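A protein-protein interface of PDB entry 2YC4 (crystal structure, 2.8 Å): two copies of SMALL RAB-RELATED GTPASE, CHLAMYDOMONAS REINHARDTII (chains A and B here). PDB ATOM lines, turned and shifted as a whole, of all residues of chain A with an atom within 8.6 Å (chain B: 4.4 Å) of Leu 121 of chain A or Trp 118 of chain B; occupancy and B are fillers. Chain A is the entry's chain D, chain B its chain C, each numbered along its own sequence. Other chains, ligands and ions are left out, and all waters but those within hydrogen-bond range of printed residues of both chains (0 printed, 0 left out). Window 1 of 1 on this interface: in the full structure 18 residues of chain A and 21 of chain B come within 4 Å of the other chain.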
ATOM      1  N   VAL A  26     -25.909 -14.458 -30.198  1.00  0.00           N
ATOM      2  CA  VAL A  26     -26.507 -15.115 -29.037  1.00  0.00           C
ATOM      3  C   VAL A  26     -27.782 -14.452 -28.555  1.00  0.00           C
ATOM      4  O   VAL A  26     -28.091 -13.342 -28.948  1.00  0.00           O
ATOM      5  CB  VAL A  26     -25.514 -15.220 -27.876  1.00  0.00           C
ATOM      6  CG1 VAL A  26     -24.464 -16.267 -28.195  1.00  0.00           C
ATOM      7  CG2 VAL A  26     -24.875 -13.878 -27.598  1.00  0.00           C
ATOM      8  N   GLY A  27     -28.518 -15.153 -27.705  1.00  0.00           N
ATOM      9  CA  GLY A  27     -29.853 -14.734 -27.332  1.00  0.00           C
ATOM     10  C   GLY A  27     -30.821 -15.881 -27.521  1.00  0.00           C
ATOM     11  O   GLY A  27     -30.593 -16.763 -28.341  1.00  0.00           O
ATOM     12  N   GLU A  28     -31.910 -15.865 -26.758  1.00  0.00           N
ATOM     13  CA  GLU A  28     -32.843 -16.986 -26.712  1.00  0.00           C
ATOM     14  C   GLU A  28     -33.368 -17.396 -28.091  1.00  0.00           C
ATOM     15  O   GLU A  28     -33.400 -16.594 -29.028  1.00  0.00           O
ATOM     16  CB  GLU A  28     -33.999 -16.677 -25.759  1.00  0.00           C
ATOM     17  CG  GLU A  28     -34.270 -17.786 -24.768  1.00  0.00           C
ATOM     18  CD  GLU A  28     -33.648 -17.535 -23.412  1.00  0.00           C
ATOM     19  OE1 GLU A  28     -34.153 -16.639 -22.692  1.00  0.00           O
ATOM     20  OE2 GLU A  28     -32.670 -18.245 -23.063  1.00  0.00           O
ATOM     21  N   THR A  80     -25.888 -19.840 -31.813  1.00  0.00           N
ATOM     22  CA  THR A  80     -25.628 -20.914 -30.853  1.00  0.00           C
ATOM     23  C   THR A  80     -26.434 -22.185 -31.191  1.00  0.00           C
ATOM     24  O   THR A  80     -25.887 -23.294 -31.308  1.00  0.00           O
ATOM     25  CB  THR A  80     -25.994 -20.489 -29.425  1.00  0.00           C
ATOM     26  OG1 THR A  80     -27.008 -21.373 -28.926  1.00  0.00           O
ATOM     27  CG2 THR A  80     -26.495 -19.020 -29.398  1.00  0.00           C
ATOM     28  N   LEU A  85     -21.856 -22.533 -32.952  1.00  0.00           N
ATOM     29  CA  LEU A  85     -20.906 -22.109 -31.936  1.00  0.00           C
ATOM     30  C   LEU A  85     -20.180 -23.326 -31.358  1.00  0.00           C
ATOM     31  O   LEU A  85     -18.940 -23.371 -31.353  1.00  0.00           O
ATOM     32  CB  LEU A  85     -21.602 -21.315 -30.838  1.00  0.00           C
ATOM     33  N   TYR A  86     -20.955 -24.320 -30.907  1.00  0.00           N
ATOM     34  CA  TYR A  86     -20.380 -25.514 -30.274  1.00  0.00           C
ATOM     35  C   TYR A  86     -19.405 -26.279 -31.176  1.00  0.00           C
ATOM     36  O   TYR A  86     -18.326 -26.667 -30.719  1.00  0.00           O
ATOM     37  CB  TYR A  86     -21.457 -26.469 -29.720  1.00  0.00           C
ATOM     38  CG  TYR A  86     -20.870 -27.685 -29.001  1.00  0.00           C
ATOM     39  CD1 TYR A  86     -20.217 -27.541 -27.792  1.00  0.00           C
ATOM     40  CD2 TYR A  86     -20.956 -28.967 -29.541  1.00  0.00           C
ATOM     41  CE1 TYR A  86     -19.671 -28.637 -27.130  1.00  0.00           C
ATOM     42  CE2 TYR A  86     -20.398 -30.076 -28.897  1.00  0.00           C
ATOM     43  CZ  TYR A  86     -19.759 -29.900 -27.688  1.00  0.00           C
ATOM     44  OH  TYR A  86     -19.209 -30.976 -27.018  1.00  0.00           O
ATOM     45  N   GLN A  89     -16.327 -24.318 -31.162  1.00  0.00           N
ATOM     46  CA  GLN A  89     -15.724 -24.317 -29.842  1.00  0.00           C
ATOM     47  C   GLN A  89     -14.858 -25.512 -29.464  1.00  0.00           C
ATOM     48  O   GLN A  89     -13.987 -25.399 -28.605  1.00  0.00           O
ATOM     49  CB  GLN A  89     -16.830 -24.220 -28.800  1.00  0.00           C
ATOM     50  CG  GLN A  89     -17.463 -22.871 -28.643  1.00  0.00           C
ATOM     51  CD  GLN A  89     -18.563 -22.903 -27.606  1.00  0.00           C
ATOM     52  OE1 GLN A  89     -19.537 -23.639 -27.749  1.00  0.00           O
ATOM     53  NE2 GLN A  89     -18.401 -22.127 -26.541  1.00  0.00           N
ATOM     54  N   VAL A  97     -14.250 -16.143 -29.056  1.00  0.00           N
ATOM     55  CA  VAL A  97     -15.149 -15.211 -29.744  1.00  0.00           C
ATOM     56  C   VAL A  97     -14.986 -13.804 -29.174  1.00  0.00           C
ATOM     57  O   VAL A  97     -15.105 -13.613 -27.972  1.00  0.00           O
ATOM     58  CB  VAL A  97     -16.626 -15.651 -29.614  1.00  0.00           C
ATOM     59  CG1 VAL A  97     -17.555 -14.461 -29.731  1.00  0.00           C
ATOM     60  CG2 VAL A  97     -16.954 -16.690 -30.677  1.00  0.00           C
ATOM     61  N   GLU A 113     -32.331 -10.419 -19.766  1.00  0.00           N
ATOM     62  CA  GLU A 113     -31.478 -10.914 -18.704  1.00  0.00           C
ATOM     63  C   GLU A 113     -30.444 -11.849 -19.289  1.00  0.00           C
ATOM     64  O   GLU A 113     -29.255 -11.696 -19.056  1.00  0.00           O
ATOM     65  CB  GLU A 113     -32.297 -11.664 -17.659  1.00  0.00           C
ATOM     66  CG  GLU A 113     -33.554 -10.947 -17.201  1.00  0.00           C
ATOM     67  CD  GLU A 113     -33.283  -9.815 -16.226  1.00  0.00           C
ATOM     68  OE1 GLU A 113     -32.234  -9.139 -16.360  1.00  0.00           O
ATOM     69  OE2 GLU A 113     -34.133  -9.604 -15.327  1.00  0.00           O
ATOM     70  N   SER A 114     -30.908 -12.825 -20.054  1.00  0.00           N
ATOM     71  CA  SER A 114     -30.031 -13.845 -20.617  1.00  0.00           C
ATOM     72  C   SER A 114     -28.896 -13.237 -21.439  1.00  0.00           C
ATOM     73  O   SER A 114     -27.773 -13.727 -21.415  1.00  0.00           O
ATOM     74  CB  SER A 114     -30.842 -14.793 -21.487  1.00  0.00           C
ATOM     75  OG  SER A 114     -30.189 -16.036 -21.602  1.00  0.00           O
ATOM     76  N   CYS A 115     -29.202 -12.170 -22.172  1.00  0.00           N
ATOM     77  CA  CYS A 115     -28.199 -11.471 -22.970  1.00  0.00           C
ATOM     78  C   CYS A 115     -27.060 -10.959 -22.121  1.00  0.00           C
ATOM     79  O   CYS A 115     -25.905 -11.063 -22.510  1.00  0.00           O
ATOM     80  CB  CYS A 115     -28.816 -10.301 -23.729  1.00  0.00           C
ATOM     81  SG  CYS A 115     -29.436 -10.806 -25.326  1.00  0.00           S
ATOM     82  N   LYS A 116     -27.411 -10.391 -20.970  1.00  0.00           N
ATOM     83  CA  LYS A 116     -26.454  -9.818 -20.040  1.00  0.00           C
ATOM     84  C   LYS A 116     -25.520 -10.864 -19.435  1.00  0.00           C
ATOM     85  O   LYS A 116     -24.315 -10.646 -19.341  1.00  0.00           O
ATOM     86  CB  LYS A 116     -27.202  -9.086 -18.937  1.00  0.00           C
ATOM     87  CG  LYS A 116     -27.837  -7.780 -19.364  1.00  0.00           C
ATOM     88  CD  LYS A 116     -28.809  -7.322 -18.308  1.00  0.00           C
ATOM     89  CE  LYS A 116     -28.921  -5.822 -18.272  1.00  0.00           C
ATOM     90  NZ  LYS A 116     -30.178  -5.375 -17.592  1.00  0.00           N
ATOM     91  N   ALA A 117     -26.068 -11.999 -19.018  1.00  0.00           N
ATOM     92  CA  ALA A 117     -25.237 -13.102 -18.542  1.00  0.00           C
ATOM     93  C   ALA A 117     -24.282 -13.579 -19.639  1.00  0.00           C
ATOM     94  O   ALA A 117     -23.070 -13.568 -19.468  1.00  0.00           O
ATOM     95  CB  ALA A 117     -26.110 -14.252 -18.027  1.00  0.00           C
ATOM     96  N   TRP A 118     -24.847 -14.001 -20.766  1.00  0.00           N
ATOM     97  CA  TRP A 118     -24.067 -14.310 -21.958  1.00  0.00           C
ATOM     98  C   TRP A 118     -22.890 -13.346 -22.078  1.00  0.00           C
ATOM     99  O   TRP A 118     -21.735 -13.734 -21.960  1.00  0.00           O
ATOM    100  CB  TRP A 118     -24.935 -14.141 -23.201  1.00  0.00           C
ATOM    101  CG  TRP A 118     -25.740 -15.341 -23.638  1.00  0.00           C
ATOM    102  CD1 TRP A 118     -27.113 -15.435 -23.692  1.00  0.00           C
ATOM    103  CD2 TRP A 118     -25.235 -16.596 -24.123  1.00  0.00           C
ATOM    104  NE1 TRP A 118     -27.485 -16.668 -24.178  1.00  0.00           N
ATOM    105  CE2 TRP A 118     -26.354 -17.400 -24.444  1.00  0.00           C
ATOM    106  CE3 TRP A 118     -23.947 -17.110 -24.335  1.00  0.00           C
ATOM    107  CZ2 TRP A 118     -26.221 -18.696 -24.954  1.00  0.00           C
ATOM    108  CZ3 TRP A 118     -23.816 -18.406 -24.836  1.00  0.00           C
ATOM    109  CH2 TRP A 118     -24.948 -19.179 -25.139  1.00  0.00           C
ATOM    110  N   PHE A 119     -23.218 -12.080 -22.307  1.00  0.00           N
ATOM    111  CA  PHE A 119     -22.250 -11.009 -22.444  1.00  0.00           C
ATOM    112  C   PHE A 119     -21.100 -11.080 -21.452  1.00  0.00           C
ATOM    113  O   PHE A 119     -19.941 -10.941 -21.818  1.00  0.00           O
ATOM    114  CB  PHE A 119     -22.952  -9.651 -22.333  1.00  0.00           C
ATOM    115  CG  PHE A 119     -22.006  -8.491 -22.312  1.00  0.00           C
ATOM    116  CD1 PHE A 119     -21.174  -8.240 -23.388  1.00  0.00           C
ATOM    117  CD2 PHE A 119     -21.924  -7.665 -21.208  1.00  0.00           C
ATOM    118  CE1 PHE A 119     -20.279  -7.183 -23.358  1.00  0.00           C
ATOM    119  CE2 PHE A 119     -21.025  -6.621 -21.176  1.00  0.00           C
ATOM    120  CZ  PHE A 119     -20.205  -6.378 -22.258  1.00  0.00           C
ATOM    121  N   GLU A 120     -21.418 -11.290 -20.187  1.00  0.00           N
ATOM    122  CA  GLU A 120     -20.386 -11.292 -19.164  1.00  0.00           C
ATOM    123  C   GLU A 120     -19.432 -12.471 -19.255  1.00  0.00           C
ATOM    124  O   GLU A 120     -18.243 -12.328 -19.004  1.00  0.00           O
ATOM    125  CB  GLU A 120     -21.002 -11.226 -17.772  1.00  0.00           C
ATOM    126  CG  GLU A 120     -21.349  -9.831 -17.360  1.00  0.00           C
ATOM    127  CD  GLU A 120     -20.133  -8.938 -17.350  1.00  0.00           C
ATOM    128  OE1 GLU A 120     -19.016  -9.450 -17.107  1.00  0.00           O
ATOM    129  OE2 GLU A 120     -20.281  -7.728 -17.596  1.00  0.00           O
ATOM    130  N   LEU A 121     -19.922 -13.647 -19.605  1.00  0.00           N
ATOM    131  CA  LEU A 121     -18.995 -14.759 -19.620  1.00  0.00           C
ATOM    132  C   LEU A 121     -18.328 -14.942 -20.966  1.00  0.00           C
ATOM    133  O   LEU A 121     -17.307 -15.600 -21.066  1.00  0.00           O
ATOM    134  CB  LEU A 121     -19.643 -16.036 -19.108  1.00  0.00           C
ATOM    135  CG  LEU A 121     -21.001 -16.340 -19.679  1.00  0.00           C
ATOM    136  CD1 LEU A 121     -20.865 -16.771 -21.151  1.00  0.00           C
ATOM    137  CD2 LEU A 121     -21.557 -17.431 -18.819  1.00  0.00           C
ATOM    138  N   LEU A 122     -18.908 -14.345 -21.993  1.00  0.00           N
ATOM    139  CA  LEU A 122     -18.207 -14.124 -23.247  1.00  0.00           C
ATOM    140  C   LEU A 122     -16.984 -13.247 -22.991  1.00  0.00           C
ATOM    141  O   LEU A 122     -15.936 -13.420 -23.611  1.00  0.00           O
ATOM    142  CB  LEU A 122     -19.131 -13.443 -24.252  1.00  0.00           C
ATOM    143  CG  LEU A 122     -20.101 -14.384 -24.950  1.00  0.00           C
ATOM    144  CD1 LEU A 122     -21.034 -13.609 -25.864  1.00  0.00           C
ATOM    145  CD2 LEU A 122     -19.340 -15.461 -25.728  1.00  0.00           C
ATOM    146  N   LYS A 123     -17.123 -12.291 -22.085  1.00  0.00           N
ATOM    147  CA  LYS A 123     -15.984 -11.481 -21.698  1.00  0.00           C
ATOM    148  C   LYS A 123     -15.036 -12.336 -20.892  1.00  0.00           C
ATOM    149  O   LYS A 123     -13.827 -12.205 -20.983  1.00  0.00           O
ATOM    150  CB  LYS A 123     -16.422 -10.270 -20.873  1.00  0.00           C
ATOM    151  CG  LYS A 123     -17.106  -9.191 -21.690  1.00  0.00           C
ATOM    152  CD  LYS A 123     -17.154  -7.872 -20.956  1.00  0.00           C
ATOM    153  CE  LYS A 123     -17.787  -8.025 -19.611  1.00  0.00           C
ATOM    154  NZ  LYS A 123     -17.875  -6.722 -18.944  1.00  0.00           N
ATOM    155  N   SER A 124     -15.595 -13.217 -20.077  1.00  0.00           N
ATOM    156  CA  SER A 124     -14.768 -14.058 -19.230  1.00  0.00           C
ATOM    157  C   SER A 124     -14.103 -15.114 -20.085  1.00  0.00           C
ATOM    158  O   SER A 124     -12.968 -15.463 -19.845  1.00  0.00           O
ATOM    159  CB  SER A 124     -15.611 -14.718 -18.134  1.00  0.00           C
ATOM    160  OG  SER A 124     -16.148 -13.751 -17.246  1.00  0.00           O
ATOM    161  N   ALA A 125     -14.816 -15.609 -21.090  1.00  0.00           N
ATOM    162  CA  ALA A 125     -14.366 -16.770 -21.828  1.00  0.00           C
ATOM    163  C   ALA A 125     -13.209 -16.502 -22.802  1.00  0.00           C
ATOM    164  O   ALA A 125     -12.597 -17.425 -23.318  1.00  0.00           O
ATOM    165  CB  ALA A 125     -15.548 -17.418 -22.545  1.00  0.00           C
ATOM    166  N   ARG A 126     -12.921 -15.236 -23.067  1.00  0.00           N
ATOM    167  CA  ARG A 126     -11.865 -14.861 -24.006  1.00  0.00           C
ATOM    168  C   ARG A 126     -10.539 -15.477 -23.603  1.00  0.00           C
ATOM    169  O   ARG A 126     -10.073 -15.255 -22.487  1.00  0.00           O
ATOM    170  CB  ARG A 126     -11.671 -13.350 -24.025  1.00  0.00           C
ATOM    171  CG  ARG A 126     -12.791 -12.545 -24.601  1.00  0.00           C
ATOM    172  CD  ARG A 126     -12.478 -11.094 -24.387  1.00  0.00           C
ATOM    173  NE  ARG A 126     -12.324 -10.803 -22.963  1.00  0.00           N
ATOM    174  CZ  ARG A 126     -11.519  -9.875 -22.459  1.00  0.00           C
ATOM    175  NH1 ARG A 126     -10.755  -9.143 -23.247  1.00  0.00           N
ATOM    176  NH2 ARG A 126     -11.470  -9.683 -21.158  1.00  0.00           N
ATOM    177  N   PRO A 127      -9.913 -16.249 -24.505  1.00  0.00           N
ATOM    178  CA  PRO A 127      -8.508 -16.654 -24.313  1.00  0.00           C
ATOM    179  C   PRO A 127      -7.590 -15.469 -24.012  1.00  0.00           C
ATOM    180  O   PRO A 127      -6.856 -15.491 -23.028  1.00  0.00           O
ATOM    181  CB  PRO A 127      -8.136 -17.262 -25.659  1.00  0.00           C
ATOM    182  CG  PRO A 127      -9.448 -17.836 -26.168  1.00  0.00           C
ATOM    183  CD  PRO A 127     -10.543 -16.936 -25.652  1.00  0.00           C
ATOM    184  N   LEU A 133     -13.909  -7.595 -25.844  1.00  0.00           N
ATOM    185  CA  LEU A 133     -15.113  -8.123 -26.463  1.00  0.00           C
ATOM    186  C   LEU A 133     -15.903  -6.973 -27.074  1.00  0.00           C
ATOM    187  O   LEU A 133     -16.267  -6.017 -26.389  1.00  0.00           O
ATOM    188  CB  LEU A 133     -15.984  -8.842 -25.439  1.00  0.00           C
ATOM    189  CG  LEU A 133     -17.330  -9.296 -25.979  1.00  0.00           C
ATOM    190  CD1 LEU A 133     -17.122 -10.501 -26.827  1.00  0.00           C
ATOM    191  CD2 LEU A 133     -18.226  -9.613 -24.849  1.00  0.00           C
ATOM    192  N   VAL B  26     -28.570 -23.038 -15.855  1.00  0.00           N
ATOM    193  CA  VAL B  26     -28.688 -22.498 -17.206  1.00  0.00           C
ATOM    194  C   VAL B  26     -29.493 -23.398 -18.123  1.00  0.00           C
ATOM    195  O   VAL B  26     -29.767 -24.549 -17.789  1.00  0.00           O
ATOM    196  CB  VAL B  26     -27.311 -22.218 -17.825  1.00  0.00           C
ATOM    197  CG1 VAL B  26     -26.698 -21.000 -17.161  1.00  0.00           C
ATOM    198  CG2 VAL B  26     -26.401 -23.438 -17.696  1.00  0.00           C
ATOM    199  N   GLY B  27     -29.864 -22.869 -19.281  1.00  0.00           N
ATOM    200  CA  GLY B  27     -30.772 -23.560 -20.167  1.00  0.00           C
ATOM    201  C   GLY B  27     -31.887 -22.611 -20.518  1.00  0.00           C
ATOM    202  O   GLY B  27     -32.150 -21.668 -19.771  1.00  0.00           O
ATOM    203  N   GLN B  89     -22.151 -11.540 -11.668  1.00  0.00           N
ATOM    204  CA  GLN B  89     -21.044 -11.457 -12.598  1.00  0.00           C
ATOM    205  C   GLN B  89     -20.295 -10.128 -12.651  1.00  0.00           C
ATOM    206  O   GLN B  89     -19.102 -10.117 -12.951  1.00  0.00           O
ATOM    207  CB  GLN B  89     -21.559 -11.765 -13.993  1.00  0.00           C
ATOM    208  CG  GLN B  89     -21.878 -13.211 -14.250  1.00  0.00           C
ATOM    209  CD  GLN B  89     -22.363 -13.426 -15.673  1.00  0.00           C
ATOM    210  OE1 GLN B  89     -23.401 -12.887 -16.079  1.00  0.00           O
ATOM    211  NE2 GLN B  89     -21.601 -14.191 -16.449  1.00  0.00           N
ATOM    212  N   SER B 114     -28.204 -25.693 -26.971  1.00  0.00           N
ATOM    213  CA  SER B 114     -27.883 -24.534 -26.157  1.00  0.00           C
ATOM    214  C   SER B 114     -27.132 -24.915 -24.883  1.00  0.00           C
ATOM    215  O   SER B 114     -26.201 -24.211 -24.461  1.00  0.00           O
ATOM    216  CB  SER B 114     -29.148 -23.757 -25.826  1.00  0.00           C
ATOM    217  OG  SER B 114     -28.810 -22.412 -25.526  1.00  0.00           O
ATOM    218  N   CYS B 115     -27.530 -26.037 -24.283  1.00  0.00           N
ATOM    219  CA  CYS B 115     -26.880 -26.522 -23.065  1.00  0.00           C
ATOM    220  C   CYS B 115     -25.404 -26.802 -23.297  1.00  0.00           C
ATOM    221  O   CYS B 115     -24.558 -26.526 -22.442  1.00  0.00           O
ATOM    222  CB  CYS B 115     -27.561 -27.793 -22.556  1.00  0.00           C
ATOM    223  SG  CYS B 115     -29.001 -27.505 -21.522  1.00  0.00           S
ATOM    224  N   LYS B 116     -25.109 -27.352 -24.470  1.00  0.00           N
ATOM    225  CA  LYS B 116     -23.759 -27.758 -24.831  1.00  0.00           C
ATOM    226  C   LYS B 116     -22.822 -26.574 -25.058  1.00  0.00           C
ATOM    227  O   LYS B 116     -21.678 -26.571 -24.593  1.00  0.00           O
ATOM    228  CB  LYS B 116     -23.824 -28.628 -26.075  1.00  0.00           C
ATOM    229  CG  LYS B 116     -24.287 -30.048 -25.833  1.00  0.00           C
ATOM    230  CD  LYS B 116     -24.564 -30.710 -27.150  1.00  0.00           C
ATOM    231  CE  LYS B 116     -24.371 -32.208 -27.066  1.00  0.00           C
ATOM    232  NZ  LYS B 116     -25.125 -32.853 -28.183  1.00  0.00           N
ATOM    233  N   ALA B 117     -23.306 -25.568 -25.779  1.00  0.00           N
ATOM    234  CA  ALA B 117     -22.568 -24.313 -25.907  1.00  0.00           C
ATOM    235  C   ALA B 117     -22.286 -23.666 -24.532  1.00  0.00           C
ATOM    236  O   ALA B 117     -21.122 -23.442 -24.158  1.00  0.00           O
ATOM    237  CB  ALA B 117     -23.312 -23.336 -26.832  1.00  0.00           C
ATOM    238  N   TRP B 118     -23.359 -23.363 -23.801  1.00  0.00           N
ATOM    239  CA  TRP B 118     -23.264 -22.912 -22.414  1.00  0.00           C
ATOM    240  C   TRP B 118     -22.112 -23.621 -21.727  1.00  0.00           C
ATOM    241  O   TRP B 118     -21.107 -23.001 -21.357  1.00  0.00           O
ATOM    242  CB  TRP B 118     -24.551 -23.249 -21.655  1.00  0.00           C
ATOM    243  CG  TRP B 118     -25.674 -22.215 -21.721  1.00  0.00           C
ATOM    244  CD1 TRP B 118     -26.911 -22.377 -22.288  1.00  0.00           C
ATOM    245  CD2 TRP B 118     -25.664 -20.889 -21.163  1.00  0.00           C
ATOM    246  NE1 TRP B 118     -27.658 -21.241 -22.125  1.00  0.00           N
ATOM    247  CE2 TRP B 118     -26.918 -20.311 -21.442  1.00  0.00           C
ATOM    248  CE3 TRP B 118     -24.718 -20.137 -20.455  1.00  0.00           C
ATOM    249  CZ2 TRP B 118     -27.247 -19.017 -21.037  1.00  0.00           C
ATOM    250  CZ3 TRP B 118     -25.048 -18.854 -20.065  1.00  0.00           C
ATOM    251  CH2 TRP B 118     -26.299 -18.310 -20.357  1.00  0.00           C
ATOM    252  N   PHE B 119     -22.273 -24.933 -21.600  1.00  0.00           N
ATOM    253  CA  PHE B 119     -21.313 -25.797 -20.951  1.00  0.00           C
ATOM    254  C   PHE B 119     -19.872 -25.513 -21.358  1.00  0.00           C
ATOM    255  O   PHE B 119     -18.985 -25.423 -20.523  1.00  0.00           O
ATOM    256  CB  PHE B 119     -21.641 -27.273 -21.212  1.00  0.00           C
ATOM    257  CG  PHE B 119     -20.557 -28.211 -20.734  1.00  0.00           C
ATOM    258  CD1 PHE B 119     -20.226 -28.279 -19.377  1.00  0.00           C
ATOM    259  CD2 PHE B 119     -19.840 -28.985 -21.626  1.00  0.00           C
ATOM    260  CE1 PHE B 119     -19.212 -29.116 -18.914  1.00  0.00           C
ATOM    261  CE2 PHE B 119     -18.823 -29.812 -21.169  1.00  0.00           C
ATOM    262  CZ  PHE B 119     -18.508 -29.871 -19.799  1.00  0.00           C
ATOM    263  N   GLU B 120     -19.636 -25.373 -22.647  1.00  0.00           N
ATOM    264  CA  GLU B 120     -18.285 -25.174 -23.117  1.00  0.00           C
ATOM    265  C   GLU B 120     -17.680 -23.841 -22.690  1.00  0.00           C
ATOM    266  O   GLU B 120     -16.486 -23.757 -22.394  1.00  0.00           O
ATOM    267  CB  GLU B 120     -18.219 -25.349 -24.634  1.00  0.00           C
ATOM    268  CG  GLU B 120     -18.040 -26.790 -25.079  1.00  0.00           C
ATOM    269  CD  GLU B 120     -16.813 -27.408 -24.486  1.00  0.00           C
ATOM    270  OE1 GLU B 120     -15.857 -26.652 -24.242  1.00  0.00           O
ATOM    271  OE2 GLU B 120     -16.814 -28.636 -24.223  1.00  0.00           O
ATOM    272  N   LEU B 121     -18.473 -22.786 -22.655  1.00  0.00           N
ATOM    273  CA  LEU B 121     -17.849 -21.520 -22.342  1.00  0.00           C
ATOM    274  C   LEU B 121     -17.876 -21.212 -20.868  1.00  0.00           C
ATOM    275  O   LEU B 121     -17.119 -20.364 -20.399  1.00  0.00           O
ATOM    276  CB  LEU B 121     -18.421 -20.379 -23.167  1.00  0.00           C
ATOM    277  CG  LEU B 121     -19.927 -20.317 -23.246  1.00  0.00           C
ATOM    278  CD1 LEU B 121     -20.474 -19.883 -21.930  1.00  0.00           C
ATOM    279  CD2 LEU B 121     -20.246 -19.310 -24.326  1.00  0.00           C
ATOM    280  N   LEU B 122     -18.742 -21.908 -20.143  1.00  0.00           N
ATOM    281  CA  LEU B 122     -18.621 -21.985 -18.686  1.00  0.00           C
ATOM    282  C   LEU B 122     -17.302 -22.609 -18.312  1.00  0.00           C
ATOM    283  O   LEU B 122     -16.704 -22.231 -17.308  1.00  0.00           O
ATOM    284  CB  LEU B 122     -19.749 -22.803 -18.074  1.00  0.00           C
ATOM    285  CG  LEU B 122     -21.108 -22.069 -17.986  1.00  0.00           C
ATOM    286  CD1 LEU B 122     -22.237 -22.977 -17.569  1.00  0.00           C
ATOM    287  CD2 LEU B 122     -21.044 -20.842 -17.049  1.00  0.00           C
ATOM    288  N   ALA B 125     -14.965 -19.850 -19.377  1.00  0.00           N
ATOM    289  CA  ALA B 125     -15.073 -18.644 -18.571  1.00  0.00           C
ATOM    290  C   ALA B 125     -14.445 -18.702 -17.166  1.00  0.00           C
ATOM    291  O   ALA B 125     -14.307 -17.672 -16.506  1.00  0.00           O
ATOM    292  CB  ALA B 125     -16.519 -18.195 -18.494  1.00  0.00           C
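The side-chain carboxylate (OE2) of Glu 120 of chain A lies within salt-bridge range of the side-chain amino group (NZ) of Lys 123 of chain A (2.9 Å). O of Glu 120 of chain A sits at hydrogen-bond distance from OG of Ser 124 of chain A (3.1 Å).
Of the 13 printed residues of chain B, 9 touch a printed residue of chain A. Hydrophobic or aromatic side chains of chain B that line the printed part of chain A: Ala 117, Trp 118, Leu 121, Leu 122 and Ala 125. Of the 24 printed residues of chain A, 9 touch a printed residue of chain B. Among the printed residues, 18 pairs touch across the chains. Among the printed residues, no Asp or Glu carboxylate lies within 4 Å of a Lys or Arg side-chain nitrogen of the other chain.
The side-chain amide nitrogen of Gln 89 of chain B is in hydrogen-bond range of the backbone carbonyl oxygen of Ala 117 of chain A, at 3.4 Å.
Leu 121 of chain A touches just these residues of chain B: Gln 89, Trp 118, Leu 121, Leu 122 and Ala 125. Of the printed residues of chain A, Glu 120 of chain B touches Tyr 86 and Gln 89. Of the printed residues of chain A, Leu 121 of chain B touches Gln 89 (3.8 Å), Trp 118 (3.7 Å), Leu 121 (3.2 Å) and Ala 125 (3.97 Å). Printed residues of chain B within 4 Å of Gln 89 of chain A: Ala 117, Glu 120 and Leu 121. Of the printed residues of chain B, Ser 124 of chain A touches Ala 125 (3.6 Å). Of the printed residues of chain A, Gln 89 of chain B touches Ala 117 (3.1 Å), Glu 120 (3.3 Å) and Leu 121 (3.6 Å). Glu 113 of chain A touches none of the printed residues of chain B. The nearest printed residue of chain B that does not touch Leu 121 of chain A is Val 26 of chain B (6.5 Å). The nearest residue of chain A that does not touch Trp 118 of chain B is Ser 114 of chain A (4.2 Å). The nearest printed residue of chain B that does not touch Thr 80 of chain A is Ala 117 of chain B (4.7 Å).
Among the printed residues, merely in contact across the chains: Thr 80 of chain A with Ser 114 of chain B (3.99 Å), Tyr 86 of chain A with Lys 116 of chain B (3.6 Å), Tyr 86 of chain A with Glu 120 of chain B (3.2 Å), Gln 89 of chain A with Ala 117 of chain B (3.6 Å), Gln 89 of chain A with Glu 120 of chain B (3.7 Å), Gln 89 of chain A with Leu 121 of chain B (3.8 Å), Trp 118 of chain A with Trp 118 of chain B (3.9 Å), Trp 118 of chain A with Leu 121 of chain B (3.7 Å), Glu 120 of chain A with Gln 89 of chain B (3.3 Å), Leu 121 of chain A with Gln 89 of chain B (3.6 Å), Leu 121 of chain A with Trp 118 of chain B (3.97 Å), Leu 121 of chain A with Leu 121 of chain B (3.2 Å), Leu 121 of chain A with Leu 122 of chain B (3.9 Å), Leu 121 of chain A with Ala 125 of chain B (3.7 Å), Ser 124 of chain A with Ala 125 of chain B (3.6 Å), Ala 125 of chain A with Leu 121 of chain B (3.97 Å) and Ala 125 of chain A with Ala 125 of chain B (3.8 Å).
Gln 89 of chain A touches Ala 117 of chain B, and with the chains exchanged Ala 117 of chain A touches Gln 89 of chain B. Gln 89 of chain A touches Glu 120 of chain B, and with the chains exchanged Glu 120 of chain A touches Gln 89 of chain B. Trp 118 of chain B touches its own counterpart, Trp 118 of chain A. Leu 121 of chain A touches Ala 125 of chain B, and with the chains exchanged Ala 125 of chain A touches Leu 121 of chain B. Of the 18 pairs that touch across the chains among the printed residues, 13 have their exchanged pair printed and touching as well.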
